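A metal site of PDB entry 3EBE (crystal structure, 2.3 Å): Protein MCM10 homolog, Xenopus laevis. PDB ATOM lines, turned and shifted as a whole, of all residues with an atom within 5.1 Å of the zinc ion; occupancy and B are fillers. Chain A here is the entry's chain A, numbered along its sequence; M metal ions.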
ATOM      1  N   CYS A 154      -3.685  -3.436  28.630  1.00  0.00           N
ATOM      2  CA  CYS A 154      -2.339  -3.927  28.247  1.00  0.00           C
ATOM      3  C   CYS A 154      -1.633  -4.648  29.398  1.00  0.00           C
ATOM      4  O   CYS A 154      -1.721  -4.204  30.548  1.00  0.00           O
ATOM      5  CB  CYS A 154      -1.491  -2.761  27.750  1.00  0.00           C
ATOM      6  SG  CYS A 154       0.201  -3.197  27.287  1.00  0.00           S
ATOM      7  N   ALA A 156       1.694  -5.307  29.644  1.00  0.00           N
ATOM      8  CA  ALA A 156       3.048  -4.800  29.864  1.00  0.00           C
ATOM      9  C   ALA A 156       3.114  -3.796  31.019  1.00  0.00           C
ATOM     10  O   ALA A 156       2.093  -3.396  31.538  1.00  0.00           O
ATOM     11  CB  ALA A 156       3.568  -4.183  28.576  1.00  0.00           C
ATOM     12  N   CYS A 164       0.671  -0.972  32.647  1.00  0.00           N
ATOM     13  CA  CYS A 164       0.228  -0.139  31.535  1.00  0.00           C
ATOM     14  C   CYS A 164      -1.295  -0.015  31.641  1.00  0.00           C
ATOM     15  O   CYS A 164      -1.983  -0.983  32.015  1.00  0.00           O
ATOM     16  CB  CYS A 164       0.645  -0.729  30.195  1.00  0.00           C
ATOM     17  SG  CYS A 164       0.187   0.245  28.770  1.00  0.00           S
ATOM     18  N   GLN A 166      -3.086   1.393  28.947  1.00  0.00           N
ATOM     19  CA  GLN A 166      -3.650   1.372  27.590  1.00  0.00           C
ATOM     20  C   GLN A 166      -4.599   0.210  27.335  1.00  0.00           C
ATOM     21  O   GLN A 166      -4.311  -0.943  27.681  1.00  0.00           O
ATOM     22  CB  GLN A 166      -2.562   1.364  26.538  1.00  0.00           C
ATOM     23  CG  GLN A 166      -1.642   2.569  26.629  1.00  0.00           C
ATOM     24  CD  GLN A 166      -2.219   3.788  25.919  1.00  0.00           C
ATOM     25  OE1 GLN A 166      -3.333   3.763  25.382  1.00  0.00           O
ATOM     26  NE2 GLN A 166      -1.434   4.838  25.879  1.00  0.00           N
ATOM     27  N   CYS A 176      -0.784  -3.194  24.053  1.00  0.00           N
ATOM     28  CA  CYS A 176      -1.132  -1.966  23.331  1.00  0.00           C
ATOM     29  C   CYS A 176      -0.147  -1.661  22.197  1.00  0.00           C
ATOM     30  O   CYS A 176       0.899  -2.294  22.079  1.00  0.00           O
ATOM     31  CB  CYS A 176      -1.205  -0.776  24.321  1.00  0.00           C
ATOM     32  SG  CYS A 176       0.421  -0.187  25.001  1.00  0.00           S
ATOM     33  N   HIS A 179       3.627  -1.026  23.379  1.00  0.00           N
ATOM     34  CA  HIS A 179       4.330  -2.183  23.905  1.00  0.00           C
ATOM     35  C   HIS A 179       4.496  -3.316  22.914  1.00  0.00           C
ATOM     36  O   HIS A 179       5.382  -4.137  23.104  1.00  0.00           O
ATOM     37  CB  HIS A 179       3.692  -2.659  25.196  1.00  0.00           C
ATOM     38  CG  HIS A 179       3.952  -1.757  26.354  1.00  0.00           C
ATOM     39  ND1 HIS A 179       2.956  -1.018  26.967  1.00  0.00           N
ATOM     40  CD2 HIS A 179       5.113  -1.426  26.979  1.00  0.00           C
ATOM     41  CE1 HIS A 179       3.490  -0.294  27.927  1.00  0.00           C
ATOM     42  NE2 HIS A 179       4.793  -0.530  27.959  1.00  0.00           N
HETATM   43 ZN    ZN M   1       0.956  -1.070  26.994  1.00  0.00          ZN
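The side-chain sulfur (SG) of Cys 164 lies close to the backbone NH (N) of Gln 166.
The backbone NH (N) of Cys 154 is in hydrogen-bond range of the backbone carbonyl oxygen (O) of Gln 166 (2.7 Å).
The backbone carbonyl oxygen (O) of Ala 156 is in hydrogen-bond range of the backbone NH (N) of Cys 164 (3.0 Å).
SG of Cys 154 sits close to N of Ala 156, 3.5 Å away.
Four residues have an atom within 4 Å of the zinc ion: Cys 154, Cys 164, Cys 176 and His 179.
The zinc ion is bound by ND1 of His 179 (2.0 Å).
The zinc ion is bound by SG of Cys 176 (2.2 Å).
The zinc ion is bound by SG of Cys 154, at 2.3 Å.
The side-chain sulfur (SG) of Cys 164 is bound to the zinc ion (2.3 Å).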
